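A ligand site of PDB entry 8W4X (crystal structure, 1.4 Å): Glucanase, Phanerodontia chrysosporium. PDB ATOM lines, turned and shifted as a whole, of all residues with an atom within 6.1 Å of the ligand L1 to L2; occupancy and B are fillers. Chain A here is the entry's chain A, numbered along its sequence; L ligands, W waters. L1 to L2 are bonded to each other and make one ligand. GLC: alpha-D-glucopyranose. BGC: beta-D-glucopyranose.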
ATOM      1  N   TYR A  83     -27.658  16.190  11.603  1.00  0.00           N
ATOM      2  CA  TYR A  83     -26.688  16.395  12.700  1.00  0.00           C
ATOM      3  C   TYR A  83     -26.234  17.856  12.699  1.00  0.00           C
ATOM      4  O   TYR A  83     -25.101  18.188  12.308  1.00  0.00           O
ATOM      5  CB  TYR A  83     -25.489  15.469  12.552  1.00  0.00           C
ATOM      6  CG  TYR A  83     -24.497  15.479  13.704  1.00  0.00           C
ATOM      7  CD1 TYR A  83     -24.900  15.123  14.985  1.00  0.00           C
ATOM      8  CD2 TYR A  83     -23.176  15.787  13.497  1.00  0.00           C
ATOM      9  CE1 TYR A  83     -24.006  15.085  16.048  1.00  0.00           C
ATOM     10  CE2 TYR A  83     -22.270  15.753  14.529  1.00  0.00           C
ATOM     11  CZ  TYR A  83     -22.685  15.389  15.798  1.00  0.00           C
ATOM     12  OH  TYR A  83     -21.757  15.408  16.838  1.00  0.00           O
ATOM     13  N   ASP A  89     -23.374  18.538  20.438  1.00  0.00           N
ATOM     14  CA  ASP A  89     -22.313  17.787  21.146  1.00  0.00           C
ATOM     15  C   ASP A  89     -22.086  18.377  22.531  1.00  0.00           C
ATOM     16  O   ASP A  89     -20.961  18.662  22.932  1.00  0.00           O
ATOM     17  CB  ASP A  89     -21.045  17.734  20.290  1.00  0.00           C
ATOM     18  CG  ASP A  89     -20.116  16.607  20.674  1.00  0.00           C
ATOM     19  OD1 ASP A  89     -20.572  15.529  21.076  1.00  0.00           O
ATOM     20  OD2 ASP A  89     -18.880  16.831  20.524  1.00  0.00           O
ATOM     21  N   ALA A  91     -21.959  17.537  25.616  1.00  0.00           N
ATOM     22  CA  ALA A  91     -21.153  16.947  26.679  1.00  0.00           C
ATOM     23  C   ALA A  91     -19.701  16.723  26.267  1.00  0.00           C
ATOM     24  O   ALA A  91     -18.985  16.015  26.989  1.00  0.00           O
ATOM     25  CB  ALA A  91     -21.794  15.653  27.193  1.00  0.00           C
ATOM     26  N   ALA A  92     -19.271  17.271  25.143  1.00  0.00           N
ATOM     27  CA  ALA A  92     -17.915  17.066  24.645  1.00  0.00           C
ATOM     28  C   ALA A  92     -17.509  18.294  23.881  1.00  0.00           C
ATOM     29  O   ALA A  92     -18.267  19.255  23.768  1.00  0.00           O
ATOM     30  CB  ALA A  92     -17.819  15.810  23.769  1.00  0.00           C
ATOM     31  N   SER A  95     -16.971  17.956  18.470  1.00  0.00           N
ATOM     32  CA  SER A  95     -17.890  18.077  17.350  1.00  0.00           C
ATOM     33  C   SER A  95     -18.862  19.235  17.532  1.00  0.00           C
ATOM     34  O   SER A  95     -19.978  19.235  16.991  1.00  0.00           O
ATOM     35  CB  SER A  95     -18.647  16.777  17.087  1.00  0.00           C
ATOM     36  OG  SER A  95     -17.830  15.794  16.447  1.00  0.00           O
ATOM     37  N   ASP A 135     -26.630  11.452  19.585  1.00  0.00           N
ATOM     38  CA  ASP A 135     -26.175  11.865  20.922  1.00  0.00           C
ATOM     39  C   ASP A 135     -27.122  12.797  21.657  1.00  0.00           C
ATOM     40  O   ASP A 135     -27.013  12.903  22.878  1.00  0.00           O
ATOM     41  CB  ASP A 135     -24.776  12.520  20.867  1.00  0.00           C
ATOM     42  CG  ASP A 135     -23.725  11.640  20.227  1.00  0.00           C
ATOM     43  OD1 ASP A 135     -23.826  10.388  20.308  1.00  0.00           O
ATOM     44  OD2 ASP A 135     -22.772  12.199  19.657  1.00  0.00           O
ATOM     45  N   ASN A 139     -27.824  12.506  25.708  1.00  0.00           N
ATOM     46  CA  ASN A 139     -27.269  13.528  26.576  1.00  0.00           C
ATOM     47  C   ASN A 139     -28.319  14.095  27.527  1.00  0.00           C
ATOM     48  O   ASN A 139     -27.988  14.469  28.659  1.00  0.00           O
ATOM     49  CB  ASN A 139     -26.616  14.664  25.769  1.00  0.00           C
ATOM     50  CG  ASN A 139     -25.146  14.383  25.436  1.00  0.00           C
ATOM     51  OD1 ASN A 139     -24.423  13.732  26.222  1.00  0.00           O
ATOM     52  ND2 ASN A 139     -24.690  14.841  24.282  1.00  0.00           N
ATOM     53  N   THR A 142     -28.695  11.388  30.623  1.00  0.00           N
ATOM     54  CA  THR A 142     -27.645  11.167  31.620  1.00  0.00           C
ATOM     55  C   THR A 142     -26.796  12.405  31.909  1.00  0.00           C
ATOM     56  O   THR A 142     -25.990  12.355  32.850  1.00  0.00           O
ATOM     57  CB  THR A 142     -26.673  10.042  31.206  1.00  0.00           C
ATOM     58  OG1 THR A 142     -25.915  10.453  30.066  1.00  0.00           O
ATOM     59  CG2 THR A 142     -27.392   8.738  30.895  1.00  0.00           C
ATOM     60  N   ASN A 143     -26.908  13.486  31.138  1.00  0.00           N
ATOM     61  CA  ASN A 143     -25.965  14.592  31.207  1.00  0.00           C
ATOM     62  C   ASN A 143     -26.640  15.928  31.526  1.00  0.00           C
ATOM     63  O   ASN A 143     -26.134  16.990  31.162  1.00  0.00           O
ATOM     64  CB  ASN A 143     -25.082  14.724  29.970  1.00  0.00           C
ATOM     65  CG  ASN A 143     -23.905  13.759  29.988  1.00  0.00           C
ATOM     66  OD1 ASN A 143     -23.290  13.538  31.050  1.00  0.00           O
ATOM     67  ND2 ASN A 143     -23.537  13.213  28.826  1.00  0.00           N
ATOM     68  N   HIS A 180     -26.222   3.966  23.214  1.00  0.00           N
ATOM     69  CA  HIS A 180     -25.693   2.617  23.089  1.00  0.00           C
ATOM     70  C   HIS A 180     -25.749   1.964  24.450  1.00  0.00           C
ATOM     71  O   HIS A 180     -26.125   2.577  25.458  1.00  0.00           O
ATOM     72  CB  HIS A 180     -24.274   2.618  22.494  1.00  0.00           C
ATOM     73  CG  HIS A 180     -23.242   3.320  23.317  1.00  0.00           C
ATOM     74  ND1 HIS A 180     -22.627   2.700  24.397  1.00  0.00           N
ATOM     75  CD2 HIS A 180     -22.693   4.553  23.200  1.00  0.00           C
ATOM     76  CE1 HIS A 180     -21.762   3.550  24.925  1.00  0.00           C
ATOM     77  NE2 HIS A 180     -21.780   4.667  24.210  1.00  0.00           N
ATOM     78  N   GLY A 182     -23.650   0.984  26.638  1.00  0.00           N
ATOM     79  CA  GLY A 182     -22.833   1.534  27.729  1.00  0.00           C
ATOM     80  C   GLY A 182     -23.285   2.894  28.183  1.00  0.00           C
ATOM     81  O   GLY A 182     -22.715   3.444  29.131  1.00  0.00           O
ATOM     82  N   TRP A 183     -24.305   3.463  27.549  1.00  0.00           N
ATOM     83  CA  TRP A 183     -24.753   4.823  27.833  1.00  0.00           C
ATOM     84  C   TRP A 183     -26.153   4.709  28.434  1.00  0.00           C
ATOM     85  O   TRP A 183     -26.347   5.015  29.608  1.00  0.00           O
ATOM     86  CB  TRP A 183     -24.704   5.653  26.550  1.00  0.00           C
ATOM     87  CG  TRP A 183     -24.854   7.122  26.725  1.00  0.00           C
ATOM     88  CD1 TRP A 183     -25.222   7.767  27.857  1.00  0.00           C
ATOM     89  CD2 TRP A 183     -24.606   8.120  25.739  1.00  0.00           C
ATOM     90  NE1 TRP A 183     -25.249   9.117  27.626  1.00  0.00           N
ATOM     91  CE2 TRP A 183     -24.858   9.361  26.348  1.00  0.00           C
ATOM     92  CE3 TRP A 183     -24.200   8.088  24.407  1.00  0.00           C
ATOM     93  CZ2 TRP A 183     -24.713  10.579  25.658  1.00  0.00           C
ATOM     94  CZ3 TRP A 183     -24.054   9.301  23.733  1.00  0.00           C
ATOM     95  CH2 TRP A 183     -24.319  10.511  24.358  1.00  0.00           C
ATOM     96  N   ASN A 216     -25.727   2.620  18.873  1.00  0.00           N
ATOM     97  CA  ASN A 216     -24.303   2.401  18.636  1.00  0.00           C
ATOM     98  C   ASN A 216     -23.724   3.322  17.579  1.00  0.00           C
ATOM     99  O   ASN A 216     -22.635   3.051  17.089  1.00  0.00           O
ATOM    100  CB  ASN A 216     -23.973   0.938  18.346  1.00  0.00           C
ATOM    101  CG  ASN A 216     -22.549   0.556  18.678  1.00  0.00           C
ATOM    102  OD1 ASN A 216     -22.038   0.817  19.769  1.00  0.00           O
ATOM    103  ND2 ASN A 216     -21.892  -0.105  17.734  1.00  0.00           N
ATOM    104  N   VAL A 217     -24.437   4.392  17.221  1.00  0.00           N
ATOM    105  CA  VAL A 217     -23.944   5.284  16.189  1.00  0.00           C
ATOM    106  C   VAL A 217     -22.624   5.884  16.604  1.00  0.00           C
ATOM    107  O   VAL A 217     -22.493   6.454  17.684  1.00  0.00           O
ATOM    108  CB  VAL A 217     -24.977   6.390  15.870  1.00  0.00           C
ATOM    109  CG1 VAL A 217     -24.359   7.414  14.955  1.00  0.00           C
ATOM    110  CG2 VAL A 217     -26.228   5.770  15.296  1.00  0.00           C
ATOM    111  N   ALA A 218     -21.612   5.723  15.755  1.00  0.00           N
ATOM    112  CA  ALA A 218     -20.251   6.196  15.983  1.00  0.00           C
ATOM    113  C   ALA A 218     -19.575   5.531  17.170  1.00  0.00           C
ATOM    114  O   ALA A 218     -18.538   6.019  17.637  1.00  0.00           O
ATOM    115  CB  ALA A 218     -20.187   7.739  16.121  1.00  0.00           C
ATOM    116  N   ASN A 219     -20.099   4.409  17.633  1.00  0.00           N
ATOM    117  CA  ASN A 219     -19.473   3.708  18.754  1.00  0.00           C
ATOM    118  C   ASN A 219     -18.997   2.339  18.253  1.00  0.00           C
ATOM    119  O   ASN A 219     -18.885   2.108  17.049  1.00  0.00           O
ATOM    120  CB  ASN A 219     -20.345   3.691  20.001  1.00  0.00           C
ATOM    121  CG  ASN A 219     -19.523   3.659  21.279  1.00  0.00           C
ATOM    122  OD1 ASN A 219     -19.010   2.592  21.660  1.00  0.00           O
ATOM    123  ND2 ASN A 219     -19.374   4.795  21.934  1.00  0.00           N
ATOM    124  N   ARG A 273     -10.857  -1.163  24.286  1.00  0.00           N
ATOM    125  CA  ARG A 273     -10.936   0.054  25.063  1.00  0.00           C
ATOM    126  C   ARG A 273     -10.493  -0.184  26.496  1.00  0.00           C
ATOM    127  O   ARG A 273     -10.678  -1.271  27.054  1.00  0.00           O
ATOM    128  CB  ARG A 273     -12.367   0.607  25.057  1.00  0.00           C
ATOM    129  CG  ARG A 273     -12.761   1.234  23.730  1.00  0.00           C
ATOM    130  CD  ARG A 273     -14.219   1.653  23.741  1.00  0.00           C
ATOM    131  NE  ARG A 273     -15.106   0.521  23.543  1.00  0.00           N
ATOM    132  CZ  ARG A 273     -16.413   0.637  23.294  1.00  0.00           C
ATOM    133  NH1 ARG A 273     -16.998   1.822  23.302  1.00  0.00           N
ATOM    134  NH2 ARG A 273     -17.124  -0.441  23.062  1.00  0.00           N
ATOM    135  N   TRP A 276     -15.265   2.135  29.123  1.00  0.00           N
ATOM    136  CA  TRP A 276     -16.386   2.152  28.169  1.00  0.00           C
ATOM    137  C   TRP A 276     -16.627   3.536  27.637  1.00  0.00           C
ATOM    138  O   TRP A 276     -17.081   3.677  26.486  1.00  0.00           O
ATOM    139  CB  TRP A 276     -17.670   1.620  28.825  1.00  0.00           C
ATOM    140  CG  TRP A 276     -18.583   0.908  27.896  1.00  0.00           C
ATOM    141  CD1 TRP A 276     -18.569   0.926  26.541  1.00  0.00           C
ATOM    142  CD2 TRP A 276     -19.655   0.041  28.270  1.00  0.00           C
ATOM    143  NE1 TRP A 276     -19.588   0.126  26.039  1.00  0.00           N
ATOM    144  CE2 TRP A 276     -20.250  -0.439  27.092  1.00  0.00           C
ATOM    145  CE3 TRP A 276     -20.169  -0.390  29.493  1.00  0.00           C
ATOM    146  CZ2 TRP A 276     -21.335  -1.309  27.103  1.00  0.00           C
ATOM    147  CZ3 TRP A 276     -21.233  -1.257  29.497  1.00  0.00           C
ATOM    148  CH2 TRP A 276     -21.811  -1.697  28.322  1.00  0.00           C
ATOM    149  N   GLY A 277     -16.327   4.565  28.395  1.00  0.00           N
ATOM    150  CA  GLY A 277     -16.518   5.936  27.975  1.00  0.00           C
ATOM    151  C   GLY A 277     -15.492   6.472  27.002  1.00  0.00           C
ATOM    152  O   GLY A 277     -15.582   7.657  26.661  1.00  0.00           O
ATOM    153  N   ASP A 278     -14.554   5.662  26.547  1.00  0.00           N
ATOM    154  CA  ASP A 278     -13.557   6.123  25.573  1.00  0.00           C
ATOM    155  C   ASP A 278     -14.157   5.945  24.183  1.00  0.00           C
ATOM    156  O   ASP A 278     -14.342   4.818  23.723  1.00  0.00           O
ATOM    157  CB  ASP A 278     -12.286   5.270  25.675  1.00  0.00           C
ATOM    158  CG  ASP A 278     -11.613   5.373  27.072  1.00  0.00           C
ATOM    159  OD1 ASP A 278     -12.001   6.262  27.831  1.00  0.00           O
ATOM    160  OD2 ASP A 278     -10.729   4.542  27.332  1.00  0.00           O
ATOM    161  N   TRP A 279     -14.475   7.058  23.529  1.00  0.00           N
ATOM    162  CA  TRP A 279     -15.215   7.064  22.264  1.00  0.00           C
ATOM    163  C   TRP A 279     -14.411   7.565  21.086  1.00  0.00           C
ATOM    164  O   TRP A 279     -14.856   7.428  19.947  1.00  0.00           O
ATOM    165  CB  TRP A 279     -16.516   7.909  22.393  1.00  0.00           C
ATOM    166  CG  TRP A 279     -16.295   9.269  22.962  1.00  0.00           C
ATOM    167  CD1 TRP A 279     -16.478   9.647  24.278  1.00  0.00           C
ATOM    168  CD2 TRP A 279     -15.842  10.439  22.279  1.00  0.00           C
ATOM    169  NE1 TRP A 279     -16.131  10.955  24.443  1.00  0.00           N
ATOM    170  CE2 TRP A 279     -15.745  11.471  23.229  1.00  0.00           C
ATOM    171  CE3 TRP A 279     -15.496  10.709  20.953  1.00  0.00           C
ATOM    172  CZ2 TRP A 279     -15.280  12.748  22.892  1.00  0.00           C
ATOM    173  CZ3 TRP A 279     -15.058  12.005  20.631  1.00  0.00           C
ATOM    174  CH2 TRP A 279     -14.952  12.982  21.606  1.00  0.00           C
HETATM  175  C1  GLC L   1     -20.597   7.599  28.110  1.00  0.00           C
HETATM  176  C2  GLC L   1     -20.679   6.968  26.734  1.00  0.00           C
HETATM  177  C3  GLC L   1     -20.069   7.858  25.651  1.00  0.00           C
HETATM  178  C4  GLC L   1     -20.666   9.234  25.689  1.00  0.00           C
HETATM  179  C5  GLC L   1     -20.569   9.819  27.111  1.00  0.00           C
HETATM  180  C6  GLC L   1     -21.359  11.070  27.077  1.00  0.00           C
HETATM  181  O1  GLC L   1     -19.263   7.678  28.560  1.00  0.00           O
HETATM  182  O2  GLC L   1     -20.030   5.689  26.677  1.00  0.00           O
HETATM  183  O3  GLC L   1     -20.352   7.186  24.369  1.00  0.00           O
HETATM  184  O4  GLC L   1     -19.888  10.119  24.873  1.00  0.00           O
HETATM  185  O5  GLC L   1     -21.136   8.923  28.035  1.00  0.00           O
HETATM  186  O6  GLC L   1     -21.009  11.788  28.372  1.00  0.00           O
HETATM  187  C2  BGC L   2     -19.642  11.676  23.092  1.00  0.00           C
HETATM  188  C3  BGC L   2     -20.079  11.972  21.694  1.00  0.00           C
HETATM  189  C4  BGC L   2     -19.905  10.727  20.814  1.00  0.00           C
HETATM  190  C5  BGC L   2     -20.624   9.550  21.420  1.00  0.00           C
HETATM  191  C6  BGC L   2     -20.342   8.275  20.683  1.00  0.00           C
HETATM  192  C1  BGC L   2     -20.385  10.476  23.615  1.00  0.00           C
HETATM  193  O2  BGC L   2     -19.932  12.788  23.938  1.00  0.00           O
HETATM  194  O3  BGC L   2     -19.253  13.033  21.101  1.00  0.00           O
HETATM  195  O4  BGC L   2     -20.322  11.006  19.482  1.00  0.00           O
HETATM  196  O5  BGC L   2     -20.101   9.360  22.762  1.00  0.00           O
HETATM  197  O6  BGC L   2     -20.995   7.176  21.300  1.00  0.00           O
HETATM  198  C2  BGC L   3     -18.307  14.867  12.938  1.00  0.00           C
HETATM  199  C3  BGC L   3     -19.076  15.197  11.683  1.00  0.00           C
HETATM  200  C4  BGC L   3     -19.077  14.064  10.704  1.00  0.00           C
HETATM  201  C5  BGC L   3     -19.538  12.815  11.322  1.00  0.00           C
HETATM  202  C6  BGC L   3     -19.428  11.613  10.431  1.00  0.00           C
HETATM  203  C1  BGC L   3     -18.834  13.571  13.573  1.00  0.00           C
HETATM  204  O1  BGC L   3     -18.142  13.137  14.616  1.00  0.00           O
HETATM  205  O2  BGC L   3     -18.498  15.900  13.889  1.00  0.00           O
HETATM  206  O3  BGC L   3     -18.491  16.375  11.067  1.00  0.00           O
HETATM  207  O4  BGC L   3     -20.045  14.409   9.676  1.00  0.00           O
HETATM  208  O5  BGC L   3     -18.762  12.509  12.510  1.00  0.00           O
HETATM  209  O6  BGC L   3     -18.045  11.261  10.225  1.00  0.00           O
HETATM  210  O   HOH W   1     -17.012  15.006  20.657  1.00  0.00           O
HETATM  211  O   HOH W   2     -21.799  14.995  23.569  1.00  0.00           O
HETATM  212  O   HOH W   3     -16.643   9.617  28.095  1.00  0.00           O
HETATM  213  O   HOH W   4     -23.061  10.413  30.626  1.00  0.00           O
HETATM  214  O   HOH W   5     -20.145   4.145  28.945  1.00  0.00           O
HETATM  215  O   HOH W   6     -18.640  13.112  26.468  1.00  0.00           O
HETATM  216  O   HOH W   7     -22.100  11.357  16.620  1.00  0.00           O
HETATM  217  O   HOH W   8     -18.015   5.197  24.505  1.00  0.00           O
HETATM  218  O   HOH W   9     -23.405   6.339  20.330  1.00  0.00           O
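The side-chain carboxylate (OD2) of Asp 135 is in hydrogen-bond range of an oxygen (O4) of BGC L2, 2.7 Å away. An oxygen (O3) of BGC L2 sits at hydrogen-bond distance from the side-chain carboxylate of Asp 89 (2.8 Å). An oxygen (O3) of GLC L1 sits at hydrogen-bond distance from a ring nitrogen (NE2) of His 180 (2.9 Å). An oxygen (O6) of GLC L1 sits at hydrogen-bond distance from the side-chain amide nitrogen of Asn 143. ND2 of Asn 219 sits at hydrogen-bond distance from O6 of BGC L2. OG of Ser 95 is in hydrogen-bond range of O2 of BGC L3, at 2.6 Å.
The backbone carbonyl oxygen of Asp 135 is in hydrogen-bond range of the side-chain amide nitrogen of Asn 139, 3.3 Å away. The backbone NH (N) of Ser 95 sits at hydrogen-bond distance from the side-chain carboxylate (OD2) of Asp 89 (3.0 Å). ND2 of Asn 219 lies within hydrogen-bond range of NE2 of His 180, 3.3 Å away. N of Gly 182 sits at hydrogen-bond distance from ND1 of His 180 (3.0 Å). The side-chain amide nitrogen of Asn 143 lies within hydrogen-bond range of the side-chain amide oxygen of Asn 139, at 2.8 Å. The side-chain amide oxygen (OD1) of Asn 219 sits at hydrogen-bond distance from the guanidinium group (NH1) of Arg 273 (2.7 Å). The side-chain hydroxyl of Thr 142 is in hydrogen-bond range of the indole nitrogen of Trp 183, 2.9 Å away.
CB of Ala 92 touches O2 of BGC L2 (3.7 Å). CZ2 of Trp 183 touches C6 of GLC L1, at 3.7 Å. O of Val 217 touches O6 of BGC L2, at 3.98 Å. O of Trp 276 touches O2 of GLC L1 (3.6 Å). Gly 277 touches the ligand L1 to L2. Trp 279 touches the ligand L1 to L2. Hydrophobic or aromatic side chains within 4 Å of the ligand L1 to L2: Ala 92, His 180, Trp 183 and Trp 279. Within 4 Å of the ligand L1 to L2: Asp 89, Ala 92, Asp 135, Asn 143, His 180, Trp 183, Val 217, Asn 219, Trp 276, Gly 277 and Trp 279.
Water W9 bridges an oxygen (O6) of BGC L2 and the backbone carbonyl oxygen of Val 217. Water W6 bridges an oxygen (O2) of BGC L2 and the backbone carbonyl oxygen of Ala 91. Water W2 lies within hydrogen-bond range of OD1 of Asp 89 (2.8 Å), O2 of BGC L2 (2.9 Å), ND2 of Asn 139 (3.0 Å) and N of Ala 91 (3.3 Å). Water W1 lies within hydrogen-bond range of the side-chain carboxylate of Asp 89 (2.6 Å) and an oxygen (O3) of BGC L2 (3.0 Å). Water W4 lies within hydrogen-bond range of the side-chain hydroxyl of Thr 142, the side-chain amide oxygen of Asn 143 and an oxygen (O6) of GLC L1. Water W7 bridges OD2 of Asp 135 (3.2 Å) and O4 of BGC L2 (3.4 Å).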
